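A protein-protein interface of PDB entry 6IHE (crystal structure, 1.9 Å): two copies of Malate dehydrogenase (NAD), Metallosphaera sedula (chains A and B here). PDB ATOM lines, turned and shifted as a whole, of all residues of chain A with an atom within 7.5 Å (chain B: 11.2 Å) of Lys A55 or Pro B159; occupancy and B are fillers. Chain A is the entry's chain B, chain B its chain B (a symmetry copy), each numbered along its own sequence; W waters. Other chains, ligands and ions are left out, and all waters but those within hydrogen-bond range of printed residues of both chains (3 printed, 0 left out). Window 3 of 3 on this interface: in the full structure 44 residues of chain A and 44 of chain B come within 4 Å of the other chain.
Asp A26 touches none of the printed residues of chain B. Of chain B, only Thr B161 comes within 4 Å of Gly A53. Lys A55 touches two residues of chain B. No residue of chain B comes within 4 Å of Ala A56. No residue of chain B comes within 4 Å of Asn A57. Arg B149 touches none of the printed residues of chain A. Pro B159 touches just one residue of chain A: Lys A55. Of the printed residues of chain A, Val B160 touches Ala A50 and Ile A54. Of the printed residues of chain A, Thr B161 touches Gly A53 and Lys A55. The nearest residue of chain B that does not touch Lys A55 is Val B160 (4.9 Å).
Printed residues of chain B that touch a printed residue of chain A: Met B146, Ser B150, Lys B154, Pro B159, Val B160 and Thr B161. Hydrophobic or aromatic side chains of chain B within 4 Å of the printed part of chain A: Met B146, Pro B159 and Val B160. Hydrophobic or aromatic side chains of chain A that line the printed part of chain B: Ala A50.
No position is printed for both chains. Of the 8 pairs that touch across the chains among the printed residues, none has its exchanged pair printed and touching as well.
Water W2 bridges NZ of Lys A55 (2.8 Å) and OG1 of Thr B161 (3.3 Å). Water W3 bridges the backbone carbonyl oxygen of Ser B150 (2.8 Å) and the guanidinium group of Arg A46 (3.2 Å). Water W1 lies within hydrogen-bond range of O of Ala A50 and NH2 of Arg B149.
Among the printed residues, merely in contact across the chains: Arg A46 with Ser B150 (3.7 Å), Arg A46 with Lys B154 (3.4 Å), Ala A50 with Met B146 (3.7 Å), Ala A50 with Val B160 (3.7 Å), Gly A53 with Thr B161 (3.6 Å), Ile A54 with Val B160 (3.7 Å), Lys A55 with Pro B159 (3.9 Å) and Lys A55 with Thr B161 (3.5 Å).
The guanidinium group (NH2) of Arg A46 is in hydrogen-bond range of the backbone carbonyl oxygen (O) of Val A58, at 2.9 Å. O of Met B146 sits at hydrogen-bond distance from OG of Ser B150, at 3.0 Å. The backbone NH (N) of Ile A54 is in hydrogen-bond range of the backbone carbonyl oxygen (O) of Phe A49, at 3.1 Å.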
ATOM      1  N   VAL A  25       7.499   6.708 -37.420  1.00  0.00           N
ATOM      2  CA  VAL A  25       8.318   5.613 -36.994  1.00  0.00           C
ATOM      3  C   VAL A  25       7.556   4.291 -37.129  1.00  0.00           C
ATOM      4  O   VAL A  25       6.583   4.065 -36.443  1.00  0.00           O
ATOM      5  CB  VAL A  25       8.790   5.851 -35.592  1.00  0.00           C
ATOM      6  CG1 VAL A  25       9.574   4.624 -35.075  1.00  0.00           C
ATOM      7  CG2 VAL A  25       9.635   7.152 -35.509  1.00  0.00           C
ATOM      8  N   ASP A  26       7.994   3.410 -38.013  1.00  0.00           N
ATOM      9  CA  ASP A  26       7.341   2.101 -38.175  1.00  0.00           C
ATOM     10  C   ASP A  26       7.776   1.092 -37.131  1.00  0.00           C
ATOM     11  O   ASP A  26       7.016   0.171 -36.775  1.00  0.00           O
ATOM     12  CB  ASP A  26       7.684   1.540 -39.527  1.00  0.00           C
ATOM     13  CG  ASP A  26       7.181   2.431 -40.665  1.00  0.00           C
ATOM     14  OD1 ASP A  26       6.013   2.871 -40.625  1.00  0.00           O
ATOM     15  OD2 ASP A  26       7.962   2.736 -41.572  1.00  0.00           O
ATOM     16  N   GLU A  27       9.010   1.203 -36.693  1.00  0.00           N
ATOM     17  CA  GLU A  27       9.582   0.326 -35.697  1.00  0.00           C
ATOM     18  C   GLU A  27      10.560   1.112 -34.912  1.00  0.00           C
ATOM     19  O   GLU A  27      11.274   1.882 -35.454  1.00  0.00           O
ATOM     20  CB  GLU A  27      10.363  -0.835 -36.300  1.00  0.00           C
ATOM     21  CG  GLU A  27       9.632  -1.651 -37.312  1.00  0.00           C
ATOM     22  CD  GLU A  27      10.397  -2.887 -37.684  1.00  0.00           C
ATOM     23  OE1 GLU A  27      11.111  -3.396 -36.840  1.00  0.00           O
ATOM     24  OE2 GLU A  27      10.300  -3.296 -38.823  1.00  0.00           O
ATOM     25  N   ARG A  46       3.059   1.199 -25.377  1.00  0.00           N
ATOM     26  CA  ARG A  46       2.033   0.274 -25.793  1.00  0.00           C
ATOM     27  C   ARG A  46       0.638   0.694 -25.322  1.00  0.00           C
ATOM     28  O   ARG A  46      -0.346   0.459 -26.017  1.00  0.00           O
ATOM     29  CB  ARG A  46       2.312  -1.157 -25.268  1.00  0.00           C
ATOM     30  CG  ARG A  46       3.394  -1.917 -26.043  1.00  0.00           C
ATOM     31  CD  ARG A  46       3.730  -3.294 -25.394  1.00  0.00           C
ATOM     32  NE  ARG A  46       4.872  -3.786 -26.145  1.00  0.00           N
ATOM     33  CZ  ARG A  46       4.849  -4.266 -27.392  1.00  0.00           C
ATOM     34  NH1 ARG A  46       3.708  -4.498 -28.047  1.00  0.00           N
ATOM     35  NH2 ARG A  46       6.014  -4.544 -27.988  1.00  0.00           N
ATOM     36  N   PHE A  49      -0.462   3.522 -27.479  1.00  0.00           N
ATOM     37  CA  PHE A  49      -0.805   3.038 -28.807  1.00  0.00           C
ATOM     38  C   PHE A  49      -2.189   2.419 -28.881  1.00  0.00           C
ATOM     39  O   PHE A  49      -2.850   2.537 -29.912  1.00  0.00           O
ATOM     40  CB  PHE A  49       0.190   1.997 -29.317  1.00  0.00           C
ATOM     41  CG  PHE A  49       1.617   2.504 -29.556  1.00  0.00           C
ATOM     42  CD1 PHE A  49       1.949   3.841 -29.486  1.00  0.00           C
ATOM     43  CD2 PHE A  49       2.632   1.580 -29.905  1.00  0.00           C
ATOM     44  CE1 PHE A  49       3.243   4.260 -29.718  1.00  0.00           C
ATOM     45  CE2 PHE A  49       3.930   2.013 -30.182  1.00  0.00           C
ATOM     46  CZ  PHE A  49       4.216   3.339 -30.061  1.00  0.00           C
ATOM     47  N   ALA A  50      -2.612   1.712 -27.828  1.00  0.00           N
ATOM     48  CA  ALA A  50      -3.893   1.030 -27.897  1.00  0.00           C
ATOM     49  C   ALA A  50      -5.071   2.001 -28.194  1.00  0.00           C
ATOM     50  O   ALA A  50      -6.023   1.672 -29.003  1.00  0.00           O
ATOM     51  CB  ALA A  50      -4.142   0.316 -26.576  1.00  0.00           C
ATOM     52  N   LYS A  52      -4.865   4.968 -29.694  1.00  0.00           N
ATOM     53  CA  LYS A  52      -4.652   5.572 -31.015  1.00  0.00           C
ATOM     54  C   LYS A  52      -4.736   4.532 -32.180  1.00  0.00           C
ATOM     55  O   LYS A  52      -4.888   4.894 -33.307  1.00  0.00           O
ATOM     56  CB  LYS A  52      -3.340   6.344 -31.042  1.00  0.00           C
ATOM     57  CG  LYS A  52      -3.224   7.610 -30.179  1.00  0.00           C
ATOM     58  CD  LYS A  52      -3.278   8.871 -31.061  1.00  0.00           C
ATOM     59  CE  LYS A  52      -3.314  10.177 -30.278  1.00  0.00           C
ATOM     60  NZ  LYS A  52      -4.583  10.788 -29.720  1.00  0.00           N
ATOM     61  N   GLY A  53      -4.758   3.228 -31.923  1.00  0.00           N
ATOM     62  CA  GLY A  53      -4.700   2.229 -33.025  1.00  0.00           C
ATOM     63  C   GLY A  53      -3.317   2.177 -33.697  1.00  0.00           C
ATOM     64  O   GLY A  53      -3.222   1.745 -34.828  1.00  0.00           O
ATOM     65  N   ILE A  54      -2.260   2.571 -32.980  1.00  0.00           N
ATOM     66  CA  ILE A  54      -0.885   2.539 -33.487  1.00  0.00           C
ATOM     67  C   ILE A  54      -0.298   1.129 -33.320  1.00  0.00           C
ATOM     68  O   ILE A  54      -0.392   0.513 -32.254  1.00  0.00           O
ATOM     69  CB  ILE A  54      -0.004   3.532 -32.779  1.00  0.00           C
ATOM     70  CG1 ILE A  54      -0.401   4.968 -33.201  1.00  0.00           C
ATOM     71  CG2 ILE A  54       1.471   3.318 -33.187  1.00  0.00           C
ATOM     72  CD1 ILE A  54       0.118   6.004 -32.244  1.00  0.00           C
ATOM     73  N   LYS A  55       0.264   0.630 -34.419  1.00  0.00           N
ATOM     74  CA  LYS A  55       0.710  -0.752 -34.555  1.00  0.00           C
ATOM     75  C   LYS A  55       2.226  -0.822 -34.747  1.00  0.00           C
ATOM     76  O   LYS A  55       2.747  -1.924 -34.912  1.00  0.00           O
ATOM     77  CB  LYS A  55      -0.034  -1.398 -35.741  1.00  0.00           C
ATOM     78  CG  LYS A  55      -1.463  -1.742 -35.408  1.00  0.00           C
ATOM     79  CD  LYS A  55      -2.267  -2.115 -36.625  1.00  0.00           C
ATOM     80  CE  LYS A  55      -2.691  -0.833 -37.356  1.00  0.00           C
ATOM     81  NZ  LYS A  55      -3.443  -1.256 -38.542  1.00  0.00           N
ATOM     82  N   ALA A  56       2.936   0.312 -34.687  1.00  0.00           N
ATOM     83  CA  ALA A  56       4.388   0.301 -34.733  1.00  0.00           C
ATOM     84  C   ALA A  56       5.001  -0.684 -33.744  1.00  0.00           C
ATOM     85  O   ALA A  56       4.563  -0.754 -32.589  1.00  0.00           O
ATOM     86  CB  ALA A  56       4.943   1.664 -34.451  1.00  0.00           C
ATOM     87  N   ASN A  57       6.007  -1.447 -34.172  1.00  0.00           N
ATOM     88  CA  ASN A  57       6.703  -2.382 -33.222  1.00  0.00           C
ATOM     89  C   ASN A  57       7.593  -1.584 -32.371  1.00  0.00           C
ATOM     90  O   ASN A  57       8.265  -0.688 -32.844  1.00  0.00           O
ATOM     91  CB  ASN A  57       7.634  -3.394 -33.891  1.00  0.00           C
ATOM     92  CG  ASN A  57       6.942  -4.311 -34.839  1.00  0.00           C
ATOM     93  OD1 ASN A  57       6.011  -5.030 -34.467  1.00  0.00           O
ATOM     94  ND2 ASN A  57       7.428  -4.342 -36.086  1.00  0.00           N
ATOM     95  N   VAL A  58       7.600  -1.894 -31.107  1.00  0.00           N
ATOM     96  CA  VAL A  58       8.408  -1.171 -30.184  1.00  0.00           C
ATOM     97  C   VAL A  58       9.029  -2.136 -29.196  1.00  0.00           C
ATOM     98  O   VAL A  58       8.370  -3.051 -28.713  1.00  0.00           O
ATOM     99  CB  VAL A  58       7.563  -0.055 -29.506  1.00  0.00           C
ATOM    100  CG1 VAL A  58       6.508  -0.619 -28.580  1.00  0.00           C
ATOM    101  CG2 VAL A  58       8.459   0.880 -28.774  1.00  0.00           C
ATOM    102  N   MET B 146      -7.105   0.184 -21.777  1.00  0.00           N
ATOM    103  CA  MET B 146      -6.085   0.182 -22.756  1.00  0.00           C
ATOM    104  C   MET B 146      -4.885  -0.691 -22.399  1.00  0.00           C
ATOM    105  O   MET B 146      -4.215  -1.266 -23.285  1.00  0.00           O
ATOM    106  CB  MET B 146      -5.708   1.608 -23.091  1.00  0.00           C
ATOM    107  CG  MET B 146      -6.845   2.351 -23.777  1.00  0.00           C
ATOM    108  SD  MET B 146      -7.428   1.649 -25.309  1.00  0.00           S
ATOM    109  CE  MET B 146      -8.923   2.577 -25.617  1.00  0.00           C
ATOM    110  N   MET B 148      -5.156  -3.439 -20.680  1.00  0.00           N
ATOM    111  CA  MET B 148      -5.683  -4.773 -20.888  1.00  0.00           C
ATOM    112  C   MET B 148      -5.619  -5.168 -22.356  1.00  0.00           C
ATOM    113  O   MET B 148      -5.186  -6.212 -22.693  1.00  0.00           O
ATOM    114  CB  MET B 148      -7.105  -4.807 -20.392  1.00  0.00           C
ATOM    115  CG  MET B 148      -7.875  -6.072 -20.693  1.00  0.00           C
ATOM    116  SD  MET B 148      -8.591  -6.228 -22.311  1.00  0.00           S
ATOM    117  CE  MET B 148      -9.978  -5.163 -22.264  1.00  0.00           C
ATOM    118  N   ARG B 149      -6.068  -4.295 -23.221  1.00  0.00           N
ATOM    119  CA  ARG B 149      -6.016  -4.518 -24.632  1.00  0.00           C
ATOM    120  C   ARG B 149      -4.600  -4.759 -25.107  1.00  0.00           C
ATOM    121  O   ARG B 149      -4.346  -5.715 -25.782  1.00  0.00           O
ATOM    122  CB  ARG B 149      -6.622  -3.329 -25.345  1.00  0.00           C
ATOM    123  CG  ARG B 149      -8.036  -3.602 -25.722  1.00  0.00           C
ATOM    124  CD  ARG B 149      -9.019  -2.523 -25.419  1.00  0.00           C
ATOM    125  NE  ARG B 149      -9.325  -1.867 -26.640  1.00  0.00           N
ATOM    126  CZ  ARG B 149     -10.458  -1.291 -26.971  1.00  0.00           C
ATOM    127  NH1 ARG B 149     -11.485  -1.249 -26.183  1.00  0.00           N
ATOM    128  NH2 ARG B 149     -10.539  -0.745 -28.144  1.00  0.00           N
ATOM    129  N   SER B 150      -3.691  -3.881 -24.741  1.00  0.00           N
ATOM    130  CA  SER B 150      -2.315  -3.982 -25.130  1.00  0.00           C
ATOM    131  C   SER B 150      -1.619  -5.265 -24.658  1.00  0.00           C
ATOM    132  O   SER B 150      -0.815  -5.802 -25.345  1.00  0.00           O
ATOM    133  CB  SER B 150      -1.556  -2.739 -24.693  1.00  0.00           C
ATOM    134  OG  SER B 150      -1.573  -2.609 -23.319  1.00  0.00           O
ATOM    135  N   PHE B 151      -1.956  -5.727 -23.476  1.00  0.00           N
ATOM    136  CA  PHE B 151      -1.393  -6.932 -22.899  1.00  0.00           C
ATOM    137  C   PHE B 151      -1.805  -8.116 -23.701  1.00  0.00           C
ATOM    138  O   PHE B 151      -0.932  -8.869 -24.119  1.00  0.00           O
ATOM    139  CB  PHE B 151      -1.761  -7.159 -21.443  1.00  0.00           C
ATOM    140  CG  PHE B 151      -1.138  -8.415 -20.850  1.00  0.00           C
ATOM    141  CD1 PHE B 151       0.171  -8.427 -20.468  1.00  0.00           C
ATOM    142  CD2 PHE B 151      -1.884  -9.592 -20.729  1.00  0.00           C
ATOM    143  CE1 PHE B 151       0.761  -9.580 -19.901  1.00  0.00           C
ATOM    144  CE2 PHE B 151      -1.327 -10.747 -20.186  1.00  0.00           C
ATOM    145  CZ  PHE B 151      -0.004 -10.741 -19.759  1.00  0.00           C
ATOM    146  N   ILE B 152      -3.101  -8.280 -23.902  1.00  0.00           N
ATOM    147  CA  ILE B 152      -3.636  -9.351 -24.752  1.00  0.00           C
ATOM    148  C   ILE B 152      -3.014  -9.366 -26.171  1.00  0.00           C
ATOM    149  O   ILE B 152      -2.638 -10.442 -26.685  1.00  0.00           O
ATOM    150  CB  ILE B 152      -5.154  -9.340 -24.815  1.00  0.00           C
ATOM    151  CG1 ILE B 152      -5.728  -9.706 -23.442  1.00  0.00           C
ATOM    152  CG2 ILE B 152      -5.678 -10.328 -25.849  1.00  0.00           C
ATOM    153  CD1 ILE B 152      -7.233  -9.525 -23.306  1.00  0.00           C
ATOM    154  N   ALA B 153      -2.866  -8.204 -26.791  1.00  0.00           N
ATOM    155  CA  ALA B 153      -2.216  -8.147 -28.079  1.00  0.00           C
ATOM    156  C   ALA B 153      -0.725  -8.646 -28.061  1.00  0.00           C
ATOM    157  O   ALA B 153      -0.336  -9.404 -28.920  1.00  0.00           O
ATOM    158  CB  ALA B 153      -2.279  -6.756 -28.670  1.00  0.00           C
ATOM    159  N   LYS B 154       0.101  -8.147 -27.165  1.00  0.00           N
ATOM    160  CA  LYS B 154       1.502  -8.526 -27.096  1.00  0.00           C
ATOM    161  C   LYS B 154       1.565 -10.039 -26.766  1.00  0.00           C
ATOM    162  O   LYS B 154       2.339 -10.751 -27.356  1.00  0.00           O
ATOM    163  CB  LYS B 154       2.212  -7.707 -26.034  1.00  0.00           C
ATOM    164  CG  LYS B 154       3.708  -7.902 -25.831  1.00  0.00           C
ATOM    165  CD  LYS B 154       4.193  -6.889 -24.800  1.00  0.00           C
ATOM    166  CE  LYS B 154       5.646  -7.045 -24.375  1.00  0.00           C
ATOM    167  NZ  LYS B 154       5.750  -7.955 -23.187  1.00  0.00           N
ATOM    168  N   LYS B 155       0.697 -10.527 -25.885  1.00  0.00           N
ATOM    169  CA  LYS B 155       0.649 -11.935 -25.508  1.00  0.00           C
ATOM    170  C   LYS B 155       0.404 -12.859 -26.697  1.00  0.00           C
ATOM    171  O   LYS B 155       1.121 -13.829 -26.848  1.00  0.00           O
ATOM    172  CB  LYS B 155      -0.437 -12.151 -24.488  1.00  0.00           C
ATOM    173  CG  LYS B 155      -0.561 -13.540 -23.917  1.00  0.00           C
ATOM    174  CD  LYS B 155       0.524 -13.773 -22.896  1.00  0.00           C
ATOM    175  CE  LYS B 155       0.340 -15.124 -22.249  1.00  0.00           C
ATOM    176  NZ  LYS B 155       1.544 -15.297 -21.396  1.00  0.00           N
ATOM    177  N   LEU B 156      -0.618 -12.574 -27.510  1.00  0.00           N
ATOM    178  CA  LEU B 156      -0.987 -13.375 -28.666  1.00  0.00           C
ATOM    179  C   LEU B 156      -0.193 -12.967 -29.900  1.00  0.00           C
ATOM    180  O   LEU B 156      -0.388 -13.530 -30.956  1.00  0.00           O
ATOM    181  CB  LEU B 156      -2.486 -13.249 -28.953  1.00  0.00           C
ATOM    182  CG  LEU B 156      -3.361 -13.657 -27.771  1.00  0.00           C
ATOM    183  CD1 LEU B 156      -4.825 -13.353 -28.016  1.00  0.00           C
ATOM    184  CD2 LEU B 156      -3.151 -15.152 -27.452  1.00  0.00           C
ATOM    185  N   LYS B 157       0.694 -11.998 -29.778  1.00  0.00           N
ATOM    186  CA  LYS B 157       1.473 -11.516 -30.912  1.00  0.00           C
ATOM    187  C   LYS B 157       0.536 -11.102 -32.048  1.00  0.00           C
ATOM    188  O   LYS B 157       0.689 -11.564 -33.193  1.00  0.00           O
ATOM    189  CB  LYS B 157       2.504 -12.596 -31.382  1.00  0.00           C
ATOM    190  CG  LYS B 157       3.226 -13.322 -30.239  1.00  0.00           C
ATOM    191  CD  LYS B 157       4.453 -14.168 -30.659  1.00  0.00           C
ATOM    192  CE  LYS B 157       5.227 -14.671 -29.426  1.00  0.00           C
ATOM    193  NZ  LYS B 157       6.365 -15.599 -29.708  1.00  0.00           N
ATOM    194  N   ILE B 158      -0.456 -10.257 -31.721  1.00  0.00           N
ATOM    195  CA  ILE B 158      -1.410  -9.697 -32.697  1.00  0.00           C
ATOM    196  C   ILE B 158      -1.433  -8.161 -32.589  1.00  0.00           C
ATOM    197  O   ILE B 158      -0.968  -7.600 -31.596  1.00  0.00           O
ATOM    198  CB  ILE B 158      -2.839 -10.262 -32.560  1.00  0.00           C
ATOM    199  CG1 ILE B 158      -3.409 -10.033 -31.170  1.00  0.00           C
ATOM    200  CG2 ILE B 158      -2.848 -11.752 -32.927  1.00  0.00           C
ATOM    201  CD1 ILE B 158      -4.818 -10.565 -30.969  1.00  0.00           C
ATOM    202  N   PRO B 159      -1.898  -7.481 -33.650  1.00  0.00           N
ATOM    203  CA  PRO B 159      -2.048  -6.024 -33.602  1.00  0.00           C
ATOM    204  C   PRO B 159      -3.049  -5.668 -32.512  1.00  0.00           C
ATOM    205  O   PRO B 159      -4.037  -6.385 -32.345  1.00  0.00           O
ATOM    206  CB  PRO B 159      -2.591  -5.663 -34.950  1.00  0.00           C
ATOM    207  CG  PRO B 159      -2.496  -6.865 -35.798  1.00  0.00           C
ATOM    208  CD  PRO B 159      -2.294  -8.054 -34.933  1.00  0.00           C
ATOM    209  N   VAL B 160      -2.744  -4.649 -31.721  1.00  0.00           N
ATOM    210  CA  VAL B 160      -3.709  -4.147 -30.658  1.00  0.00           C
ATOM    211  C   VAL B 160      -5.106  -3.783 -31.186  1.00  0.00           C
ATOM    212  O   VAL B 160      -6.134  -4.021 -30.522  1.00  0.00           O
ATOM    213  CB  VAL B 160      -3.070  -2.995 -29.842  1.00  0.00           C
ATOM    214  CG1 VAL B 160      -2.945  -1.734 -30.708  1.00  0.00           C
ATOM    215  CG2 VAL B 160      -3.842  -2.761 -28.557  1.00  0.00           C
ATOM    216  N   THR B 161      -5.152  -3.369 -32.453  1.00  0.00           N
ATOM    217  CA  THR B 161      -6.386  -3.080 -33.148  1.00  0.00           C
ATOM    218  C   THR B 161      -7.327  -4.306 -33.377  1.00  0.00           C
ATOM    219  O   THR B 161      -8.468  -4.138 -33.754  1.00  0.00           O
ATOM    220  CB  THR B 161      -6.081  -2.479 -34.466  1.00  0.00           C
ATOM    221  OG1 THR B 161      -5.201  -3.376 -35.175  1.00  0.00           O
ATOM    222  CG2 THR B 161      -5.405  -1.088 -34.264  1.00  0.00           C
ATOM    223  N   SER B 162      -6.807  -5.514 -33.162  1.00  0.00           N
ATOM    224  CA  SER B 162      -7.597  -6.788 -33.149  1.00  0.00           C
ATOM    225  C   SER B 162      -8.354  -7.052 -31.870  1.00  0.00           C
ATOM    226  O   SER B 162      -9.192  -7.957 -31.818  1.00  0.00           O
ATOM    227  CB  SER B 162      -6.624  -7.992 -33.361  1.00  0.00           C
ATOM    228  OG  SER B 162      -6.368  -8.003 -34.717  1.00  0.00           O
ATOM    229  N   VAL B 163      -8.009  -6.299 -30.822  1.00  0.00           N
ATOM    230  CA  VAL B 163      -8.591  -6.498 -29.486  1.00  0.00           C
ATOM    231  C   VAL B 163      -9.591  -5.381 -29.108  1.00  0.00           C
ATOM    232  O   VAL B 163      -9.322  -4.175 -29.301  1.00  0.00           O
ATOM    233  CB  VAL B 163      -7.493  -6.574 -28.415  1.00  0.00           C
ATOM    234  CG1 VAL B 163      -8.065  -7.050 -27.082  1.00  0.00           C
ATOM    235  CG2 VAL B 163      -6.378  -7.506 -28.890  1.00  0.00           C
ATOM    236  N   ASP B 164     -10.738  -5.811 -28.590  1.00  0.00           N
ATOM    237  CA  ASP B 164     -11.843  -4.978 -28.159  1.00  0.00           C
ATOM    238  C   ASP B 164     -12.184  -5.374 -26.744  1.00  0.00           C
ATOM    239  O   ASP B 164     -11.894  -6.466 -26.343  1.00  0.00           O
ATOM    240  CB  ASP B 164     -13.069  -5.211 -29.029  1.00  0.00           C
ATOM    241  CG  ASP B 164     -13.923  -3.946 -29.234  1.00  0.00           C
ATOM    242  OD1 ASP B 164     -13.944  -3.090 -28.368  1.00  0.00           O
ATOM    243  OD2 ASP B 164     -14.582  -3.819 -30.260  1.00  0.00           O
ATOM    244  N   GLY B 165     -12.811  -4.470 -26.005  1.00  0.00           N
ATOM    245  CA  GLY B 165     -13.206  -4.750 -24.650  1.00  0.00           C
ATOM    246  C   GLY B 165     -12.857  -3.718 -23.620  1.00  0.00           C
ATOM    247  O   GLY B 165     -12.118  -2.808 -23.863  1.00  0.00           O
ATOM    248  N   VAL B 182     -14.677  -8.465 -23.965  1.00  0.00           N
ATOM    249  CA  VAL B 182     -13.344  -8.679 -24.537  1.00  0.00           C
ATOM    250  C   VAL B 182     -13.461  -9.663 -25.687  1.00  0.00           C
ATOM    251  O   VAL B 182     -13.945 -10.795 -25.506  1.00  0.00           O
ATOM    252  CB  VAL B 182     -12.354  -9.208 -23.502  1.00  0.00           C
ATOM    253  CG1 VAL B 182     -10.962  -9.368 -24.106  1.00  0.00           C
ATOM    254  CG2 VAL B 182     -12.318  -8.269 -22.297  1.00  0.00           C
ATOM    255  N   LYS B 183     -13.076  -9.190 -26.873  1.00  0.00           N
ATOM    256  CA  LYS B 183     -13.193  -9.949 -28.113  1.00  0.00           C
ATOM    257  C   LYS B 183     -11.912  -9.776 -28.933  1.00  0.00           C
ATOM    258  O   LYS B 183     -11.315  -8.675 -28.924  1.00  0.00           O
ATOM    259  CB  LYS B 183     -14.362  -9.468 -28.973  1.00  0.00           C
ATOM    260  CG  LYS B 183     -15.747  -9.383 -28.330  1.00  0.00           C
ATOM    261  CD  LYS B 183     -16.403 -10.722 -28.115  1.00  0.00           C
ATOM    262  CE  LYS B 183     -17.607 -10.626 -27.165  1.00  0.00           C
ATOM    263  NZ  LYS B 183     -18.903 -10.584 -27.881  1.00  0.00           N
ATOM    264  N   ILE B 184     -11.495 -10.847 -29.627  1.00  0.00           N
ATOM    265  CA  ILE B 184     -10.325 -10.832 -30.512  1.00  0.00           C
ATOM    266  C   ILE B 184     -10.889 -11.125 -31.893  1.00  0.00           C
ATOM    267  O   ILE B 184     -11.501 -12.165 -32.106  1.00  0.00           O
ATOM    268  CB  ILE B 184      -9.229 -11.850 -30.140  1.00  0.00           C
ATOM    269  CG1 ILE B 184      -8.568 -11.498 -28.816  1.00  0.00           C
ATOM    270  CG2 ILE B 184      -8.104 -11.831 -31.192  1.00  0.00           C
ATOM    271  CD1 ILE B 184      -9.229 -12.154 -27.646  1.00  0.00           C
ATOM    272  N   LYS B 185     -10.743 -10.155 -32.795  1.00  0.00           N
ATOM    273  CA  LYS B 185     -11.357 -10.201 -34.121  1.00  0.00           C
ATOM    274  C   LYS B 185     -12.800 -10.638 -34.082  1.00  0.00           C
ATOM    275  O   LYS B 185     -13.255 -11.336 -34.970  1.00  0.00           O
ATOM    276  CB  LYS B 185     -10.510 -11.071 -35.080  1.00  0.00           C
ATOM    277  CG  LYS B 185      -9.126 -10.480 -35.366  1.00  0.00           C
ATOM    278  CD  LYS B 185      -8.432 -11.033 -36.612  1.00  0.00           C
ATOM    279  CE  LYS B 185      -8.681 -10.213 -37.865  1.00  0.00           C
ATOM    280  NZ  LYS B 185      -8.393  -8.765 -37.798  1.00  0.00           N
ATOM    281  N   GLY B 186     -13.531 -10.174 -33.068  1.00  0.00           N
ATOM    282  CA  GLY B 186     -14.941 -10.471 -32.938  1.00  0.00           C
ATOM    283  C   GLY B 186     -15.250 -11.708 -32.125  1.00  0.00           C
ATOM    284  O   GLY B 186     -16.387 -11.940 -31.779  1.00  0.00           O
ATOM    285  N   PHE B 192      -9.352 -18.267 -27.085  1.00  0.00           N
ATOM    286  CA  PHE B 192      -7.915 -18.072 -27.205  1.00  0.00           C
ATOM    287  C   PHE B 192      -7.248 -18.505 -25.935  1.00  0.00           C
ATOM    288  O   PHE B 192      -7.877 -18.722 -24.908  1.00  0.00           O
ATOM    289  CB  PHE B 192      -7.589 -16.602 -27.496  1.00  0.00           C
ATOM    290  CG  PHE B 192      -8.113 -16.148 -28.819  1.00  0.00           C
ATOM    291  CD1 PHE B 192      -9.464 -15.878 -28.975  1.00  0.00           C
ATOM    292  CD2 PHE B 192      -7.276 -16.048 -29.914  1.00  0.00           C
ATOM    293  CE1 PHE B 192      -9.977 -15.495 -30.197  1.00  0.00           C
ATOM    294  CE2 PHE B 192      -7.782 -15.661 -31.138  1.00  0.00           C
ATOM    295  CZ  PHE B 192      -9.130 -15.377 -31.283  1.00  0.00           C
HETATM  296  O   HOH W   1      -8.777   2.068 -29.227  1.00  0.00           O
HETATM  297  O   HOH W   2      -5.958  -2.372 -38.231  1.00  0.00           O
HETATM  298  O   HOH W   3       0.692  -4.185 -27.035  1.00  0.00           O
